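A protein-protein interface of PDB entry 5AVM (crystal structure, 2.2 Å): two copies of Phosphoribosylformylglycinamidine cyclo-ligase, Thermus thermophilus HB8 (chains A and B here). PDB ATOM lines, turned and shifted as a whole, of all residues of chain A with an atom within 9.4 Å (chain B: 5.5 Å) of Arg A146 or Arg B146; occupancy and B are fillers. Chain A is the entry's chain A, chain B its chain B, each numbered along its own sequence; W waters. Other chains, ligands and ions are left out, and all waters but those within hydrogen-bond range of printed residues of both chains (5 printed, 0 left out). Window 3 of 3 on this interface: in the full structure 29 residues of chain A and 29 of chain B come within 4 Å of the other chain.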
ATOM      1  N   LEU A  68      25.268 -20.481 -19.232  1.00  0.00           N
ATOM      2  CA  LEU A  68      25.055 -21.383 -18.106  1.00  0.00           C
ATOM      3  C   LEU A  68      24.469 -22.733 -18.524  1.00  0.00           C
ATOM      4  O   LEU A  68      24.839 -23.776 -17.982  1.00  0.00           O
ATOM      5  CB  LEU A  68      24.161 -20.704 -17.067  1.00  0.00           C
ATOM      6  CG  LEU A  68      24.784 -19.479 -16.386  1.00  0.00           C
ATOM      7  CD1 LEU A  68      23.772 -18.838 -15.439  1.00  0.00           C
ATOM      8  CD2 LEU A  68      26.045 -19.899 -15.636  1.00  0.00           C
ATOM      9  N   LEU A  71      27.222 -24.684 -20.315  1.00  0.00           N
ATOM     10  CA  LEU A  71      28.166 -25.202 -19.331  1.00  0.00           C
ATOM     11  C   LEU A  71      27.558 -26.424 -18.648  1.00  0.00           C
ATOM     12  O   LEU A  71      28.188 -27.479 -18.551  1.00  0.00           O
ATOM     13  CB  LEU A  71      28.468 -24.135 -18.278  1.00  0.00           C
ATOM     14  CG  LEU A  71      29.362 -22.948 -18.635  1.00  0.00           C
ATOM     15  CD1 LEU A  71      29.404 -21.983 -17.458  1.00  0.00           C
ATOM     16  CD2 LEU A  71      30.765 -23.444 -18.966  1.00  0.00           C
ATOM     17  N   ALA A 106      35.207 -13.944 -18.666  1.00  0.00           N
ATOM     18  CA  ALA A 106      35.467 -13.867 -17.234  1.00  0.00           C
ATOM     19  C   ALA A 106      34.814 -15.056 -16.531  1.00  0.00           C
ATOM     20  O   ALA A 106      33.848 -15.624 -17.031  1.00  0.00           O
ATOM     21  CB  ALA A 106      34.940 -12.561 -16.676  1.00  0.00           C
ATOM     22  N   ALA A 107      35.337 -15.436 -15.370  1.00  0.00           N
ATOM     23  CA  ALA A 107      34.787 -16.580 -14.659  1.00  0.00           C
ATOM     24  C   ALA A 107      35.248 -16.668 -13.222  1.00  0.00           C
ATOM     25  O   ALA A 107      36.224 -16.024 -12.836  1.00  0.00           O
ATOM     26  CB  ALA A 107      35.181 -17.846 -15.375  1.00  0.00           C
ATOM     27  N   SER A 108      34.537 -17.478 -12.438  1.00  0.00           N
ATOM     28  CA  SER A 108      34.891 -17.707 -11.042  1.00  0.00           C
ATOM     29  C   SER A 108      36.265 -18.353 -11.118  1.00  0.00           C
ATOM     30  O   SER A 108      37.165 -18.049 -10.336  1.00  0.00           O
ATOM     31  CB  SER A 108      33.892 -18.670 -10.386  1.00  0.00           C
ATOM     32  OG  SER A 108      34.283 -19.019  -9.069  1.00  0.00           O
ATOM     33  N   HIS A 109      36.413 -19.243 -12.091  1.00  0.00           N
ATOM     34  CA  HIS A 109      37.664 -19.948 -12.325  1.00  0.00           C
ATOM     35  C   HIS A 109      37.742 -20.316 -13.811  1.00  0.00           C
ATOM     36  O   HIS A 109      36.795 -20.868 -14.374  1.00  0.00           O
ATOM     37  CB  HIS A 109      37.747 -21.201 -11.442  1.00  0.00           C
ATOM     38  CG  HIS A 109      39.026 -21.959 -11.601  1.00  0.00           C
ATOM     39  ND1 HIS A 109      39.150 -23.041 -12.446  1.00  0.00           N
ATOM     40  CD2 HIS A 109      40.254 -21.755 -11.070  1.00  0.00           C
ATOM     41  CE1 HIS A 109      40.400 -23.470 -12.430  1.00  0.00           C
ATOM     42  NE2 HIS A 109      41.091 -22.706 -11.602  1.00  0.00           N
ATOM     43  N   MET A 141      37.767 -14.130 -11.577  1.00  0.00           N
ATOM     44  CA  MET A 141      37.362 -13.402 -10.383  1.00  0.00           C
ATOM     45  C   MET A 141      36.327 -14.149  -9.546  1.00  0.00           C
ATOM     46  O   MET A 141      35.142 -13.807  -9.567  1.00  0.00           O
ATOM     47  CB  MET A 141      36.808 -12.033 -10.787  1.00  0.00           C
ATOM     48  CG  MET A 141      37.733 -11.236 -11.705  1.00  0.00           C
ATOM     49  SD  MET A 141      37.188  -9.539 -11.930  1.00  0.00           S
ATOM     50  CE  MET A 141      36.172  -9.699 -13.376  1.00  0.00           C
ATOM     51  N   PRO A 142      36.768 -15.167  -8.778  1.00  0.00           N
ATOM     52  CA  PRO A 142      35.880 -15.971  -7.927  1.00  0.00           C
ATOM     53  C   PRO A 142      35.106 -15.124  -6.921  1.00  0.00           C
ATOM     54  O   PRO A 142      34.149 -15.594  -6.297  1.00  0.00           O
ATOM     55  CB  PRO A 142      36.839 -16.946  -7.253  1.00  0.00           C
ATOM     56  CG  PRO A 142      38.118 -16.155  -7.170  1.00  0.00           C
ATOM     57  CD  PRO A 142      38.180 -15.520  -8.537  1.00  0.00           C
ATOM     58  N   GLY A 143      35.525 -13.870  -6.766  1.00  0.00           N
ATOM     59  CA  GLY A 143      34.844 -12.979  -5.850  1.00  0.00           C
ATOM     60  C   GLY A 143      33.715 -12.257  -6.561  1.00  0.00           C
ATOM     61  O   GLY A 143      32.826 -11.675  -5.926  1.00  0.00           O
ATOM     62  N   VAL A 144      33.745 -12.302  -7.892  1.00  0.00           N
ATOM     63  CA  VAL A 144      32.732 -11.637  -8.712  1.00  0.00           C
ATOM     64  C   VAL A 144      31.697 -12.607  -9.276  1.00  0.00           C
ATOM     65  O   VAL A 144      30.504 -12.304  -9.323  1.00  0.00           O
ATOM     66  CB  VAL A 144      33.403 -10.866  -9.881  1.00  0.00           C
ATOM     67  CG1 VAL A 144      32.356 -10.427 -10.902  1.00  0.00           C
ATOM     68  CG2 VAL A 144      34.153  -9.655  -9.329  1.00  0.00           C
ATOM     69  N   TYR A 145      32.169 -13.777  -9.691  1.00  0.00           N
ATOM     70  CA  TYR A 145      31.312 -14.798 -10.273  1.00  0.00           C
ATOM     71  C   TYR A 145      30.932 -15.916  -9.316  1.00  0.00           C
ATOM     72  O   TYR A 145      31.717 -16.308  -8.449  1.00  0.00           O
ATOM     73  CB  TYR A 145      31.993 -15.386 -11.516  1.00  0.00           C
ATOM     74  CG  TYR A 145      31.970 -14.431 -12.688  1.00  0.00           C
ATOM     75  CD1 TYR A 145      30.838 -14.323 -13.495  1.00  0.00           C
ATOM     76  CD2 TYR A 145      33.042 -13.572 -12.939  1.00  0.00           C
ATOM     77  CE1 TYR A 145      30.765 -13.383 -14.515  1.00  0.00           C
ATOM     78  CE2 TYR A 145      32.977 -12.624 -13.959  1.00  0.00           C
ATOM     79  CZ  TYR A 145      31.830 -12.536 -14.741  1.00  0.00           C
ATOM     80  OH  TYR A 145      31.736 -11.590 -15.741  1.00  0.00           O
ATOM     81  N   ARG A 146      29.706 -16.408  -9.469  1.00  0.00           N
ATOM     82  CA  ARG A 146      29.229 -17.509  -8.655  1.00  0.00           C
ATOM     83  C   ARG A 146      30.018 -18.684  -9.196  1.00  0.00           C
ATOM     84  O   ARG A 146      30.393 -18.688 -10.370  1.00  0.00           O
ATOM     85  CB  ARG A 146      27.720 -17.721  -8.850  1.00  0.00           C
ATOM     86  CG  ARG A 146      26.878 -16.584  -8.277  1.00  0.00           C
ATOM     87  CD  ARG A 146      25.385 -16.888  -8.272  1.00  0.00           C
ATOM     88  NE  ARG A 146      24.637 -15.938  -7.440  1.00  0.00           N
ATOM     89  CZ  ARG A 146      24.710 -15.871  -6.106  1.00  0.00           C
ATOM     90  NH1 ARG A 146      25.496 -16.702  -5.430  1.00  0.00           N
ATOM     91  NH2 ARG A 146      24.002 -14.961  -5.444  1.00  0.00           N
ATOM     92  N   GLU A 147      30.297 -19.664  -8.346  1.00  0.00           N
ATOM     93  CA  GLU A 147      31.066 -20.828  -8.761  1.00  0.00           C
ATOM     94  C   GLU A 147      30.535 -21.450 -10.050  1.00  0.00           C
ATOM     95  O   GLU A 147      29.334 -21.682 -10.198  1.00  0.00           O
ATOM     96  CB  GLU A 147      31.094 -21.850  -7.623  1.00  0.00           C
ATOM     97  CG  GLU A 147      31.861 -21.335  -6.404  1.00  0.00           C
ATOM     98  CD  GLU A 147      31.846 -22.299  -5.227  1.00  0.00           C
ATOM     99  OE1 GLU A 147      32.212 -23.485  -5.418  1.00  0.00           O
ATOM    100  OE2 GLU A 147      31.479 -21.864  -4.108  1.00  0.00           O
ATOM    101  N   GLY A 148      31.442 -21.695 -10.992  1.00  0.00           N
ATOM    102  CA  GLY A 148      31.057 -22.280 -12.264  1.00  0.00           C
ATOM    103  C   GLY A 148      30.503 -21.272 -13.259  1.00  0.00           C
ATOM    104  O   GLY A 148      30.393 -21.558 -14.451  1.00  0.00           O
ATOM    105  N   ALA A 149      30.159 -20.087 -12.775  1.00  0.00           N
ATOM    106  CA  ALA A 149      29.601 -19.055 -13.632  1.00  0.00           C
ATOM    107  C   ALA A 149      30.650 -18.432 -14.540  1.00  0.00           C
ATOM    108  O   ALA A 149      31.795 -18.204 -14.133  1.00  0.00           O
ATOM    109  CB  ALA A 149      28.940 -17.977 -12.784  1.00  0.00           C
ATOM    110  N   TRP A 150      30.243 -18.166 -15.781  1.00  0.00           N
ATOM    111  CA  TRP A 150      31.090 -17.543 -16.799  1.00  0.00           C
ATOM    112  C   TRP A 150      30.262 -16.470 -17.483  1.00  0.00           C
ATOM    113  O   TRP A 150      29.040 -16.421 -17.325  1.00  0.00           O
ATOM    114  CB  TRP A 150      31.490 -18.541 -17.896  1.00  0.00           C
ATOM    115  CG  TRP A 150      32.645 -19.450 -17.623  1.00  0.00           C
ATOM    116  CD1 TRP A 150      32.660 -20.533 -16.800  1.00  0.00           C
ATOM    117  CD2 TRP A 150      33.940 -19.391 -18.237  1.00  0.00           C
ATOM    118  NE1 TRP A 150      33.879 -21.159 -16.866  1.00  0.00           N
ATOM    119  CE2 TRP A 150      34.685 -20.476 -17.740  1.00  0.00           C
ATOM    120  CE3 TRP A 150      34.542 -18.521 -19.161  1.00  0.00           C
ATOM    121  CZ2 TRP A 150      36.008 -20.720 -18.133  1.00  0.00           C
ATOM    122  CZ3 TRP A 150      35.857 -18.761 -19.552  1.00  0.00           C
ATOM    123  CH2 TRP A 150      36.573 -19.853 -19.037  1.00  0.00           C
ATOM    124  N   ASP A 151      30.937 -15.617 -18.247  1.00  0.00           N
ATOM    125  CA  ASP A 151      30.267 -14.589 -19.028  1.00  0.00           C
ATOM    126  C   ASP A 151      31.083 -14.398 -20.288  1.00  0.00           C
ATOM    127  O   ASP A 151      32.270 -14.102 -20.227  1.00  0.00           O
ATOM    128  CB  ASP A 151      30.148 -13.262 -18.278  1.00  0.00           C
ATOM    129  CG  ASP A 151      29.352 -12.220 -19.066  1.00  0.00           C
ATOM    130  OD1 ASP A 151      28.296 -12.572 -19.640  1.00  0.00           O
ATOM    131  OD2 ASP A 151      29.775 -11.045 -19.114  1.00  0.00           O
ATOM    132  N   ARG A 194      15.966 -22.003 -19.218  1.00  0.00           N
ATOM    133  CA  ARG A 194      16.556 -22.808 -18.154  1.00  0.00           C
ATOM    134  C   ARG A 194      15.648 -23.153 -16.971  1.00  0.00           C
ATOM    135  O   ARG A 194      15.821 -24.203 -16.350  1.00  0.00           O
ATOM    136  CB  ARG A 194      17.836 -22.139 -17.640  1.00  0.00           C
ATOM    137  CG  ARG A 194      19.015 -22.192 -18.609  1.00  0.00           C
ATOM    138  CD  ARG A 194      20.297 -21.733 -17.927  1.00  0.00           C
ATOM    139  NE  ARG A 194      20.106 -20.441 -17.277  1.00  0.00           N
ATOM    140  CZ  ARG A 194      20.195 -20.229 -15.967  1.00  0.00           C
ATOM    141  NH1 ARG A 194      20.483 -21.225 -15.137  1.00  0.00           N
ATOM    142  NH2 ARG A 194      19.971 -19.016 -15.485  1.00  0.00           N
ATOM    143  N   SER B 108      24.928  -8.356 -10.756  1.00  0.00           N
ATOM    144  CA  SER B 108      23.894  -9.204 -10.181  1.00  0.00           C
ATOM    145  C   SER B 108      22.618  -8.380 -10.323  1.00  0.00           C
ATOM    146  O   SER B 108      21.565  -8.881 -10.720  1.00  0.00           O
ATOM    147  CB  SER B 108      24.190  -9.468  -8.705  1.00  0.00           C
ATOM    148  OG  SER B 108      23.143 -10.194  -8.094  1.00  0.00           O
ATOM    149  N   PRO B 142      21.652 -12.242 -12.346  1.00  0.00           N
ATOM    150  CA  PRO B 142      21.798 -12.650 -10.950  1.00  0.00           C
ATOM    151  C   PRO B 142      22.126 -14.131 -10.848  1.00  0.00           C
ATOM    152  O   PRO B 142      22.463 -14.632  -9.775  1.00  0.00           O
ATOM    153  CB  PRO B 142      20.441 -12.296 -10.349  1.00  0.00           C
ATOM    154  CG  PRO B 142      19.507 -12.410 -11.519  1.00  0.00           C
ATOM    155  CD  PRO B 142      20.291 -11.741 -12.606  1.00  0.00           C
ATOM    156  N   GLY B 143      22.039 -14.826 -11.976  1.00  0.00           N
ATOM    157  CA  GLY B 143      22.342 -16.244 -11.988  1.00  0.00           C
ATOM    158  C   GLY B 143      23.806 -16.495 -12.283  1.00  0.00           C
ATOM    159  O   GLY B 143      24.284 -17.628 -12.177  1.00  0.00           O
ATOM    160  N   VAL B 144      24.520 -15.433 -12.649  1.00  0.00           N
ATOM    161  CA  VAL B 144      25.948 -15.518 -12.969  1.00  0.00           C
ATOM    162  C   VAL B 144      26.838 -14.804 -11.939  1.00  0.00           C
ATOM    163  O   VAL B 144      27.930 -15.280 -11.612  1.00  0.00           O
ATOM    164  CB  VAL B 144      26.230 -14.910 -14.381  1.00  0.00           C
ATOM    165  CG1 VAL B 144      27.729 -14.875 -14.658  1.00  0.00           C
ATOM    166  CG2 VAL B 144      25.512 -15.722 -15.454  1.00  0.00           C
ATOM    167  N   TYR B 145      26.352 -13.671 -11.430  1.00  0.00           N
ATOM    168  CA  TYR B 145      27.094 -12.850 -10.482  1.00  0.00           C
ATOM    169  C   TYR B 145      26.767 -13.033  -9.001  1.00  0.00           C
ATOM    170  O   TYR B 145      25.632 -13.337  -8.635  1.00  0.00           O
ATOM    171  CB  TYR B 145      26.904 -11.375 -10.850  1.00  0.00           C
ATOM    172  CG  TYR B 145      27.527 -11.027 -12.173  1.00  0.00           C
ATOM    173  CD1 TYR B 145      28.895 -10.776 -12.267  1.00  0.00           C
ATOM    174  CD2 TYR B 145      26.770 -11.037 -13.349  1.00  0.00           C
ATOM    175  CE1 TYR B 145      29.499 -10.549 -13.501  1.00  0.00           C
ATOM    176  CE2 TYR B 145      27.365 -10.814 -14.594  1.00  0.00           C
ATOM    177  CZ  TYR B 145      28.734 -10.572 -14.662  1.00  0.00           C
ATOM    178  OH  TYR B 145      29.347 -10.368 -15.880  1.00  0.00           O
ATOM    179  N   ARG B 146      27.786 -12.840  -8.162  1.00  0.00           N
ATOM    180  CA  ARG B 146      27.638 -12.922  -6.714  1.00  0.00           C
ATOM    181  C   ARG B 146      26.771 -11.718  -6.367  1.00  0.00           C
ATOM    182  O   ARG B 146      26.780 -10.716  -7.083  1.00  0.00           O
ATOM    183  CB  ARG B 146      29.000 -12.795  -6.013  1.00  0.00           C
ATOM    184  CG  ARG B 146      29.926 -14.006  -6.139  1.00  0.00           C
ATOM    185  CD  ARG B 146      29.303 -15.227  -5.495  1.00  0.00           C
ATOM    186  NE  ARG B 146      30.196 -16.385  -5.441  1.00  0.00           N
ATOM    187  CZ  ARG B 146      29.832 -17.575  -4.969  1.00  0.00           C
ATOM    188  NH1 ARG B 146      28.598 -17.764  -4.518  1.00  0.00           N
ATOM    189  NH2 ARG B 146      30.699 -18.578  -4.948  1.00  0.00           N
ATOM    190  N   GLU B 147      26.020 -11.813  -5.279  1.00  0.00           N
ATOM    191  CA  GLU B 147      25.149 -10.722  -4.870  1.00  0.00           C
ATOM    192  C   GLU B 147      25.904  -9.409  -4.792  1.00  0.00           C
ATOM    193  O   GLU B 147      27.001  -9.352  -4.237  1.00  0.00           O
ATOM    194  CB  GLU B 147      24.539 -11.022  -3.504  1.00  0.00           C
ATOM    195  CG  GLU B 147      23.649  -9.917  -2.978  1.00  0.00           C
ATOM    196  CD  GLU B 147      22.423  -9.721  -3.834  1.00  0.00           C
ATOM    197  OE1 GLU B 147      22.578  -9.418  -5.037  1.00  0.00           O
ATOM    198  OE2 GLU B 147      21.302  -9.875  -3.304  1.00  0.00           O
ATOM    199  N   GLY B 148      25.311  -8.355  -5.350  1.00  0.00           N
ATOM    200  CA  GLY B 148      25.927  -7.036  -5.319  1.00  0.00           C
ATOM    201  C   GLY B 148      27.171  -6.841  -6.168  1.00  0.00           C
ATOM    202  O   GLY B 148      27.714  -5.736  -6.219  1.00  0.00           O
ATOM    203  N   ALA B 149      27.618  -7.898  -6.841  1.00  0.00           N
ATOM    204  CA  ALA B 149      28.812  -7.832  -7.677  1.00  0.00           C
ATOM    205  C   ALA B 149      28.572  -7.214  -9.058  1.00  0.00           C
ATOM    206  O   ALA B 149      27.459  -7.248  -9.593  1.00  0.00           O
ATOM    207  CB  ALA B 149      29.422  -9.225  -7.830  1.00  0.00           C
HETATM  208  O   HOH W   1      31.554  -9.456 -18.323  1.00  0.00           O
HETATM  209  O   HOH W   2      33.436 -17.805  -6.947  1.00  0.00           O
HETATM  210  O   HOH W   3      22.539 -17.435  -8.020  1.00  0.00           O
HETATM  211  O   HOH W   4      22.913 -12.588  -7.617  1.00  0.00           O
HETATM  212  O   HOH W   5      29.395 -20.700  -3.626  1.00  0.00           O
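The backbone carbonyl oxygen of Val A144 lies within hydrogen-bond range of the backbone NH of Arg B146, 3.0 Å away. OH of Tyr A145 sits at hydrogen-bond distance from OH of Tyr B145. The backbone carbonyl oxygen (O) of Tyr A145 is in hydrogen-bond range of the guanidinium group (NE) of Arg B146 (3.4 Å). The guanidinium group (NE) of Arg A146 lies within hydrogen-bond range of the backbone carbonyl oxygen (O) of Pro B142 (3.4 Å). The backbone NH (N) of Arg A146 is in hydrogen-bond range of the backbone carbonyl oxygen (O) of Val B144 (3.0 Å). The backbone carbonyl oxygen of Tyr B145 is in hydrogen-bond range of the guanidinium group of Arg A146, 3.0 Å away. OE2 of Glu A147 is in salt-bridge range of NH2 of Arg B146, at 3.5 Å. The side-chain carboxylate (OD2) of Asp A151 is in hydrogen-bond range of the side-chain hydroxyl (OH) of Tyr B145, 3.3 Å away. The guanidinium group (NH1) of Arg A146 sits close to the guanidinium group (NH1) of Arg B146, 3.4 Å away.
Leu A68 touches Gly B143. Val B144 touches Leu A68 (CG2 to CD1, 3.6 Å). Arg B146 touches Gly A143 (CG to O, 3.7 Å). O of Val A144 touches CA of Tyr B145, at 3.6 Å. CB of Ala B149 touches O of Val A144 (3.6 Å). Val B144 touches Tyr A145 (CG1 to CD1, 3.4 Å). Glu B147 touches Arg A146. O of Val B144 touches CB of Ala A149, at 3.1 Å. Trp A150 touches Val B144.
The backbone NH (N) of Asp A151 is in hydrogen-bond range of the backbone carbonyl oxygen (O) of Ala A106 (3.2 Å). The backbone carbonyl oxygen of Ala A149 is in hydrogen-bond range of the backbone NH of Ser A108. OG of Ser B108 is in hydrogen-bond range of OE1 of Glu B147. The backbone carbonyl oxygen of Ala B149 sits at hydrogen-bond distance from the backbone NH of Ser B108, at 3.0 Å.
Hydrophobic or aromatic side chains of chain A within 4 Å of the printed part of chain B: Leu A68, Val A144, Tyr A145 and Ala A149.
Gly A143 touches Arg B146, but with the chains exchanged Arg A146 does not touch Gly B143 (4.1 Å). Val A144 touches Ala B149, and with the chains exchanged Ala A149 touches Val B144. Tyr A145 touches its own counterpart, Tyr B145. Arg A146 touches Pro B142, but with the chains exchanged Pro A142 does not touch Arg B146 (4.1 Å).
Arg A146 touches just these residues of chain B: Pro B142, Val B144, Tyr B145, Arg B146 and Glu B147. Printed residues of chain A within 4 Å of Ala B149: Val A144 (3.6 Å). Of the printed residues of chain A, Glu B147 touches Arg A146. Of the printed residues of chain B, Val A144 touches Tyr B145, Arg B146 and Ala B149. Of the printed residues of chain A, Tyr B145 touches Val A144, Tyr A145, Arg A146 and Asp A151. Printed residues of chain A within 4 Å of Pro B142: Arg A146. Of the printed residues of chain B, Trp A150 touches Val B144. His A109 touches none of the printed residues of chain B. Pro A142 touches none of the printed residues of chain B. The nearest residue of chain A that does not touch Arg B146 is Pro A142 (4.1 Å). The nearest printed residue of chain B that does not touch Glu A147 is Val B144 (6.0 Å).
Water W2 lies within hydrogen-bond range of O of Pro A142 (2.4 Å), OG of Ser A108 (2.6 Å), O of Tyr A145 (2.7 Å) and NH2 of Arg B146 (3.5 Å). Water W5 bridges OE2 of Glu A147 (2.4 Å) and NH2 of Arg B146 (2.8 Å). Water W4 lies within hydrogen-bond range of the side-chain hydroxyl (OG) of Ser B108, the backbone carbonyl oxygen (O) of Tyr B145, the backbone carbonyl oxygen (O) of Pro B142 and the guanidinium group (NH2) of Arg A146. Water W1 lies within hydrogen-bond range of OD2 of Asp A151, OH of Tyr A145 and OH of Tyr B145. Water W3 bridges NE of Arg A146 and O of Pro B142.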
